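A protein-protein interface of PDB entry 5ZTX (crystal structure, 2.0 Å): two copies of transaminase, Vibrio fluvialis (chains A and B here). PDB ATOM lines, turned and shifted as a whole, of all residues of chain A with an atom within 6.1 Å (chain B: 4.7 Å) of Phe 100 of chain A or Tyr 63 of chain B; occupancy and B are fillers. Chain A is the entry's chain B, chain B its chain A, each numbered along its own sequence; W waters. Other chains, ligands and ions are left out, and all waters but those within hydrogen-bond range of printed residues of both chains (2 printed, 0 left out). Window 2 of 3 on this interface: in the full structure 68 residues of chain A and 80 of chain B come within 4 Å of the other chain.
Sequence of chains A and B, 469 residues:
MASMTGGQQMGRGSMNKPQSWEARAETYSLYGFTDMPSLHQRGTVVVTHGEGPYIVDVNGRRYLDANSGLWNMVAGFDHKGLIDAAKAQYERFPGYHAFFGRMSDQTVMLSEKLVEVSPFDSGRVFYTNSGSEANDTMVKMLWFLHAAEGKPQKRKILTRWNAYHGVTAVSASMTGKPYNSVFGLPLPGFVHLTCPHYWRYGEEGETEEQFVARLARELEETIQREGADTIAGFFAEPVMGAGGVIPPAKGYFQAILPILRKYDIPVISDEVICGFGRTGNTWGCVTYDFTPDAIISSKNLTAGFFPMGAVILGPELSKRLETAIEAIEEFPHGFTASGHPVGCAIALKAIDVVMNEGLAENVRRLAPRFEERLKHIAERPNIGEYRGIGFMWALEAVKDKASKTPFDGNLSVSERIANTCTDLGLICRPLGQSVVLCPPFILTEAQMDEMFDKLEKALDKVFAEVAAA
Among the printed residues, pairs that only touch across the chains: Gly 95 of chain A with Val 47 of chain B, Gly 95 of chain A with Ile 55 of chain B, His 97 of chain A with Ile 427 of chain B, Phe 99 of chain A with Ile 427 of chain B, Phe 100 of chain A with Ile 55 of chain B, Phe 100 of chain A with Tyr 63 of chain B, Phe 100 of chain A with Thr 422 of chain B, Phe 100 of chain A with Ile 427 of chain B and Gly 101 of chain A with Val 45 of chain B.
No position is printed for both chains.
Of the 11 pairs that touch across the chains among the printed residues, none has its exchanged pair printed and touching as well.
N of Asp 65 of chain B lies within hydrogen-bond range of O of Pro 53 of chain B (3.0 Å).
The backbone carbonyl oxygen of Ile 55 of chain B lies within hydrogen-bond range of the backbone NH of Tyr 63 of chain B, at 2.7 Å.
The side-chain hydroxyl (OH) of Tyr 63 of chain B sits at hydrogen-bond distance from the side-chain carboxylate (OD2) of Asp 57 of chain B, 2.6 Å away.
O of Leu 64 of chain B is in hydrogen-bond range of N of Ile 427 of chain B, at 2.8 Å.
A ring nitrogen (ND1) of His 97 of chain A sits at hydrogen-bond distance from the backbone NH of Phe 99 of chain A.
The backbone NH of Phe 100 of chain A is in hydrogen-bond range of a ring nitrogen (ND1) of His 97 of chain A.
Water W2 lies within hydrogen-bond range of O of Arg 102 of chain A and O of Val 47 of chain B.
Water W1 bridges N of Gly 95 of chain A (3.0 Å) and O of Val 47 of chain B (3.1 Å).
Of the 14 printed residues of chain B, 7 touch a printed residue of chain A.
Printed residues of chain B that touch a printed residue of chain A: Val 45, Val 47, Ile 55, Tyr 63, Asp 65, Thr 422 and Ile 427.
Hydrophobic or aromatic side chains of chain B within 4 Å of the printed part of chain A: Val 47, Ile 55, Tyr 63 and Ile 427.
Of the printed residues of chain B, Phe 100 of chain A touches Ile 55 (3.8 Å), Tyr 63 (3.7 Å), Thr 422 (3.6 Å) and Ile 427 (3.6 Å).
Arg 62 of chain B touches none of the printed residues of chain A.
Tyr 63 of chain B touches just one residue of chain A: Phe 100.
Of the printed residues of chain A, Asp 65 of chain B touches His 97 (2.8 Å).
Of the printed residues of chain A, Thr 422 of chain B touches Phe 100.
Of the printed residues of chain A, Ile 427 of chain B touches His 97 (3.7 Å), Phe 99 (3.8 Å) and Phe 100 (3.6 Å).
The nearest printed residue of chain B that does not touch His 97 of chain A is Ile 55 of chain B (4.01 Å).
The backbone carbonyl oxygen of Val 45 of chain B sits at hydrogen-bond distance from the backbone NH of Arg 102 of chain A (2.9 Å).
OD1 of Asp 65 of chain B is in hydrogen-bond range of NE2 of His 97 of chain A (2.8 Å).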
ATOM      1  N   GLY A  95       2.890  33.923  -3.712  1.00  0.00           N
ATOM      2  CA  GLY A  95       3.829  33.043  -4.373  1.00  0.00           C
ATOM      3  C   GLY A  95       5.088  33.837  -4.748  1.00  0.00           C
ATOM      4  O   GLY A  95       5.502  33.903  -5.916  1.00  0.00           O
ATOM      5  N   HIS A  97       8.618  34.992  -5.557  1.00  0.00           N
ATOM      6  CA  HIS A  97       9.664  34.218  -6.173  1.00  0.00           C
ATOM      7  C   HIS A  97      10.724  35.142  -6.712  1.00  0.00           C
ATOM      8  O   HIS A  97      10.385  36.260  -7.180  1.00  0.00           O
ATOM      9  CB  HIS A  97       9.071  33.408  -7.335  1.00  0.00           C
ATOM     10  CG  HIS A  97       9.840  32.152  -7.627  1.00  0.00           C
ATOM     11  ND1 HIS A  97      10.942  32.140  -8.437  1.00  0.00           N
ATOM     12  CD2 HIS A  97       9.735  30.895  -7.127  1.00  0.00           C
ATOM     13  CE1 HIS A  97      11.497  30.933  -8.447  1.00  0.00           C
ATOM     14  NE2 HIS A  97      10.786  30.155  -7.660  1.00  0.00           N
ATOM     15  N   ALA A  98      11.950  34.621  -6.766  1.00  0.00           N
ATOM     16  CA  ALA A  98      13.103  35.348  -7.295  1.00  0.00           C
ATOM     17  C   ALA A  98      12.941  35.675  -8.789  1.00  0.00           C
ATOM     18  O   ALA A  98      13.380  36.714  -9.258  1.00  0.00           O
ATOM     19  CB  ALA A  98      14.385  34.538  -7.030  1.00  0.00           C
ATOM     20  N   PHE A  99      12.399  34.750  -9.582  1.00  0.00           N
ATOM     21  CA  PHE A  99      12.213  35.048 -11.005  1.00  0.00           C
ATOM     22  C   PHE A  99      11.003  34.422 -11.701  1.00  0.00           C
ATOM     23  O   PHE A  99      10.789  34.761 -12.829  1.00  0.00           O
ATOM     24  CB  PHE A  99      13.491  34.604 -11.782  1.00  0.00           C
ATOM     25  CG  PHE A  99      13.869  33.170 -11.515  1.00  0.00           C
ATOM     26  CD1 PHE A  99      13.308  32.142 -12.256  1.00  0.00           C
ATOM     27  CD2 PHE A  99      14.739  32.858 -10.486  1.00  0.00           C
ATOM     28  CE1 PHE A  99      13.649  30.833 -12.018  1.00  0.00           C
ATOM     29  CE2 PHE A  99      15.035  31.525 -10.178  1.00  0.00           C
ATOM     30  CZ  PHE A  99      14.527  30.517 -10.962  1.00  0.00           C
ATOM     31  N   PHE A 100      10.209  33.559 -11.060  1.00  0.00           N
ATOM     32  CA  PHE A 100       9.161  32.849 -11.765  1.00  0.00           C
ATOM     33  C   PHE A 100       7.836  33.617 -11.578  1.00  0.00           C
ATOM     34  O   PHE A 100       7.500  34.006 -10.476  1.00  0.00           O
ATOM     35  CB  PHE A 100       8.961  31.462 -11.249  1.00  0.00           C
ATOM     36  CG  PHE A 100       7.922  30.711 -12.003  1.00  0.00           C
ATOM     37  CD1 PHE A 100       8.207  30.219 -13.252  1.00  0.00           C
ATOM     38  CD2 PHE A 100       6.633  30.578 -11.518  1.00  0.00           C
ATOM     39  CE1 PHE A 100       7.232  29.579 -14.001  1.00  0.00           C
ATOM     40  CE2 PHE A 100       5.660  29.920 -12.263  1.00  0.00           C
ATOM     41  CZ  PHE A 100       5.959  29.416 -13.506  1.00  0.00           C
ATOM     42  N   GLY A 101       7.102  33.805 -12.649  1.00  0.00           N
ATOM     43  CA  GLY A 101       5.748  34.350 -12.576  1.00  0.00           C
ATOM     44  C   GLY A 101       5.756  35.852 -12.696  1.00  0.00           C
ATOM     45  O   GLY A 101       6.746  36.493 -12.416  1.00  0.00           O
ATOM     46  N   ARG A 102       4.637  36.406 -13.136  1.00  0.00           N
ATOM     47  CA  ARG A 102       4.479  37.845 -13.359  1.00  0.00           C
ATOM     48  C   ARG A 102       4.581  38.615 -12.052  1.00  0.00           C
ATOM     49  O   ARG A 102       4.257  38.087 -10.981  1.00  0.00           O
ATOM     50  CB  ARG A 102       3.117  38.099 -14.033  1.00  0.00           C
ATOM     51  CG  ARG A 102       2.800  39.549 -14.376  1.00  0.00           C
ATOM     52  CD  ARG A 102       1.444  39.676 -15.077  1.00  0.00           C
ATOM     53  NE  ARG A 102       1.414  38.855 -16.280  1.00  0.00           N
ATOM     54  CZ  ARG A 102       0.326  38.609 -17.013  1.00  0.00           C
ATOM     55  NH1 ARG A 102      -0.869  39.121 -16.701  1.00  0.00           N
ATOM     56  NH2 ARG A 102       0.438  37.817 -18.070  1.00  0.00           N
ATOM     57  N   VAL B  45       3.203  33.839 -16.621  1.00  0.00           N
ATOM     58  CA  VAL B  45       2.348  33.034 -15.744  1.00  0.00           C
ATOM     59  C   VAL B  45       1.900  33.837 -14.529  1.00  0.00           C
ATOM     60  O   VAL B  45       2.741  34.385 -13.812  1.00  0.00           O
ATOM     61  CB  VAL B  45       3.089  31.720 -15.335  1.00  0.00           C
ATOM     62  CG1 VAL B  45       2.329  30.963 -14.265  1.00  0.00           C
ATOM     63  CG2 VAL B  45       3.225  30.832 -16.564  1.00  0.00           C
ATOM     64  N   VAL B  47       0.675  34.142 -10.846  1.00  0.00           N
ATOM     65  CA  VAL B  47       0.827  33.354  -9.606  1.00  0.00           C
ATOM     66  C   VAL B  47       0.249  34.147  -8.468  1.00  0.00           C
ATOM     67  O   VAL B  47       0.550  35.382  -8.328  1.00  0.00           O
ATOM     68  CB  VAL B  47       2.305  33.090  -9.349  1.00  0.00           C
ATOM     69  CG1 VAL B  47       2.498  32.485  -7.960  1.00  0.00           C
ATOM     70  CG2 VAL B  47       2.772  32.113 -10.415  1.00  0.00           C
ATOM     71  N   PRO B  53       5.584  22.817  -1.424  1.00  0.00           N
ATOM     72  CA  PRO B  53       6.758  23.186  -2.212  1.00  0.00           C
ATOM     73  C   PRO B  53       6.400  23.668  -3.593  1.00  0.00           C
ATOM     74  O   PRO B  53       7.270  23.854  -4.421  1.00  0.00           O
ATOM     75  CB  PRO B  53       7.525  21.862  -2.271  1.00  0.00           C
ATOM     76  CG  PRO B  53       6.422  20.881  -2.344  1.00  0.00           C
ATOM     77  CD  PRO B  53       5.394  21.365  -1.407  1.00  0.00           C
ATOM     78  N   TYR B  54       5.104  23.913  -3.861  1.00  0.00           N
ATOM     79  CA  TYR B  54       4.652  24.329  -5.196  1.00  0.00           C
ATOM     80  C   TYR B  54       4.260  25.806  -5.327  1.00  0.00           C
ATOM     81  O   TYR B  54       3.555  26.345  -4.475  1.00  0.00           O
ATOM     82  CB  TYR B  54       3.417  23.517  -5.612  1.00  0.00           C
ATOM     83  CG  TYR B  54       3.625  22.033  -5.665  1.00  0.00           C
ATOM     84  CD1 TYR B  54       4.245  21.427  -6.766  1.00  0.00           C
ATOM     85  CD2 TYR B  54       3.251  21.208  -4.606  1.00  0.00           C
ATOM     86  CE1 TYR B  54       4.466  20.062  -6.808  1.00  0.00           C
ATOM     87  CE2 TYR B  54       3.500  19.845  -4.655  1.00  0.00           C
ATOM     88  CZ  TYR B  54       4.062  19.277  -5.751  1.00  0.00           C
ATOM     89  OH  TYR B  54       4.266  17.917  -5.809  1.00  0.00           O
ATOM     90  N   ILE B  55       4.715  26.440  -6.396  1.00  0.00           N
ATOM     91  CA  ILE B  55       4.098  27.656  -6.884  1.00  0.00           C
ATOM     92  C   ILE B  55       2.836  27.233  -7.620  1.00  0.00           C
ATOM     93  O   ILE B  55       2.867  26.242  -8.333  1.00  0.00           O
ATOM     94  CB  ILE B  55       5.043  28.384  -7.886  1.00  0.00           C
ATOM     95  CG1 ILE B  55       6.153  29.087  -7.121  1.00  0.00           C
ATOM     96  CG2 ILE B  55       4.300  29.447  -8.715  1.00  0.00           C
ATOM     97  CD1 ILE B  55       5.800  30.247  -6.199  1.00  0.00           C
ATOM     98  N   ASP B  57      -0.258  28.522 -10.187  1.00  0.00           N
ATOM     99  CA  ASP B  57      -0.838  29.576 -11.019  1.00  0.00           C
ATOM    100  C   ASP B  57      -2.356  29.692 -10.900  1.00  0.00           C
ATOM    101  O   ASP B  57      -3.022  28.876 -10.215  1.00  0.00           O
ATOM    102  CB  ASP B  57      -0.376  29.549 -12.507  1.00  0.00           C
ATOM    103  CG  ASP B  57      -0.989  28.414 -13.364  1.00  0.00           C
ATOM    104  OD1 ASP B  57      -2.102  27.792 -13.125  1.00  0.00           O
ATOM    105  OD2 ASP B  57      -0.305  28.150 -14.387  1.00  0.00           O
ATOM    106  N   ARG B  61      -2.267  25.140 -12.042  1.00  0.00           N
ATOM    107  CA  ARG B  61      -1.086  24.365 -12.339  1.00  0.00           C
ATOM    108  C   ARG B  61      -0.062  24.549 -11.205  1.00  0.00           C
ATOM    109  O   ARG B  61       0.223  25.659 -10.795  1.00  0.00           O
ATOM    110  CB  ARG B  61      -0.503  24.745 -13.672  1.00  0.00           C
ATOM    111  CG  ARG B  61       0.529  23.739 -14.091  1.00  0.00           C
ATOM    112  CD  ARG B  61       0.966  23.935 -15.530  1.00  0.00           C
ATOM    113  NE  ARG B  61       1.762  22.786 -15.898  1.00  0.00           N
ATOM    114  CZ  ARG B  61       2.730  22.775 -16.801  1.00  0.00           C
ATOM    115  NH1 ARG B  61       3.373  21.629 -16.997  1.00  0.00           N
ATOM    116  NH2 ARG B  61       3.077  23.872 -17.471  1.00  0.00           N
ATOM    117  N   ARG B  62       0.505  23.441 -10.775  1.00  0.00           N
ATOM    118  CA  ARG B  62       1.459  23.400  -9.687  1.00  0.00           C
ATOM    119  C   ARG B  62       2.872  23.268 -10.237  1.00  0.00           C
ATOM    120  O   ARG B  62       3.150  22.426 -11.053  1.00  0.00           O
ATOM    121  CB  ARG B  62       1.147  22.274  -8.707  1.00  0.00           C
ATOM    122  CG  ARG B  62      -0.212  22.418  -8.032  1.00  0.00           C
ATOM    123  CD  ARG B  62      -0.578  21.088  -7.361  1.00  0.00           C
ATOM    124  NE  ARG B  62      -0.678  21.130  -5.942  1.00  0.00           N
ATOM    125  CZ  ARG B  62      -0.317  20.132  -5.123  1.00  0.00           C
ATOM    126  NH1 ARG B  62      -0.458  20.314  -3.819  1.00  0.00           N
ATOM    127  NH2 ARG B  62       0.215  18.961  -5.571  1.00  0.00           N
ATOM    128  N   TYR B  63       3.755  24.114  -9.787  1.00  0.00           N
ATOM    129  CA  TYR B  63       5.119  24.110 -10.270  1.00  0.00           C
ATOM    130  C   TYR B  63       6.051  23.865  -9.092  1.00  0.00           C
ATOM    131  O   TYR B  63       6.163  24.680  -8.150  1.00  0.00           O
ATOM    132  CB  TYR B  63       5.513  25.398 -10.979  1.00  0.00           C
ATOM    133  CG  TYR B  63       4.610  25.871 -12.137  1.00  0.00           C
ATOM    134  CD1 TYR B  63       3.404  26.441 -11.875  1.00  0.00           C
ATOM    135  CD2 TYR B  63       5.025  25.810 -13.489  1.00  0.00           C
ATOM    136  CE1 TYR B  63       2.586  26.945 -12.901  1.00  0.00           C
ATOM    137  CE2 TYR B  63       4.201  26.301 -14.559  1.00  0.00           C
ATOM    138  CZ  TYR B  63       2.978  26.849 -14.224  1.00  0.00           C
ATOM    139  OH  TYR B  63       2.110  27.337 -15.091  1.00  0.00           O
ATOM    140  N   LEU B  64       6.756  22.756  -9.184  1.00  0.00           N
ATOM    141  CA  LEU B  64       7.604  22.276  -8.056  1.00  0.00           C
ATOM    142  C   LEU B  64       8.728  23.240  -8.020  1.00  0.00           C
ATOM    143  O   LEU B  64       9.386  23.476  -9.018  1.00  0.00           O
ATOM    144  CB  LEU B  64       8.077  20.815  -8.281  1.00  0.00           C
ATOM    145  CG  LEU B  64       8.890  20.188  -7.116  1.00  0.00           C
ATOM    146  CD1 LEU B  64       8.134  20.101  -5.823  1.00  0.00           C
ATOM    147  CD2 LEU B  64       9.160  18.756  -7.460  1.00  0.00           C
ATOM    148  N   ASP B  65       8.849  23.956  -6.917  1.00  0.00           N
ATOM    149  CA  ASP B  65       9.770  25.041  -6.896  1.00  0.00           C
ATOM    150  C   ASP B  65      11.125  24.613  -6.305  1.00  0.00           C
ATOM    151  O   ASP B  65      11.378  24.818  -5.131  1.00  0.00           O
ATOM    152  CB  ASP B  65       9.242  26.198  -6.119  1.00  0.00           C
ATOM    153  CG  ASP B  65      10.155  27.418  -6.184  1.00  0.00           C
ATOM    154  OD1 ASP B  65      11.145  27.458  -6.960  1.00  0.00           O
ATOM    155  OD2 ASP B  65       9.869  28.346  -5.393  1.00  0.00           O
ATOM    156  N   THR B 422      10.171  24.655 -16.692  1.00  0.00           N
ATOM    157  CA  THR B 422       8.963  25.405 -16.321  1.00  0.00           C
ATOM    158  C   THR B 422       7.720  24.886 -17.138  1.00  0.00           C
ATOM    159  O   THR B 422       6.650  24.518 -16.542  1.00  0.00           O
ATOM    160  CB  THR B 422       9.332  26.890 -16.484  1.00  0.00           C
ATOM    161  OG1 THR B 422       9.798  27.369 -15.207  1.00  0.00           O
ATOM    162  CG2 THR B 422       8.286  27.691 -16.976  1.00  0.00           C
ATOM    163  N   GLY B 425       6.485  21.988 -15.461  1.00  0.00           N
ATOM    164  CA  GLY B 425       6.053  22.167 -14.081  1.00  0.00           C
ATOM    165  C   GLY B 425       7.147  22.036 -13.012  1.00  0.00           C
ATOM    166  O   GLY B 425       6.878  21.544 -11.933  1.00  0.00           O
ATOM    167  N   ILE B 427      10.503  24.464 -11.445  1.00  0.00           N
ATOM    168  CA  ILE B 427      11.217  25.669 -11.495  1.00  0.00           C
ATOM    169  C   ILE B 427      12.631  25.390 -11.002  1.00  0.00           C
ATOM    170  O   ILE B 427      12.795  24.859  -9.867  1.00  0.00           O
ATOM    171  CB  ILE B 427      10.620  26.736 -10.565  1.00  0.00           C
ATOM    172  CG1 ILE B 427       9.183  27.068 -10.970  1.00  0.00           C
ATOM    173  CG2 ILE B 427      11.412  28.031 -10.698  1.00  0.00           C
ATOM    174  CD1 ILE B 427       8.496  27.827  -9.848  1.00  0.00           C
HETATM  175  O   HOH W   1       1.857  35.965  -5.589  1.00  0.00           O
HETATM  176  O   HOH W   2       1.814  36.794 -10.516  1.00  0.00           O
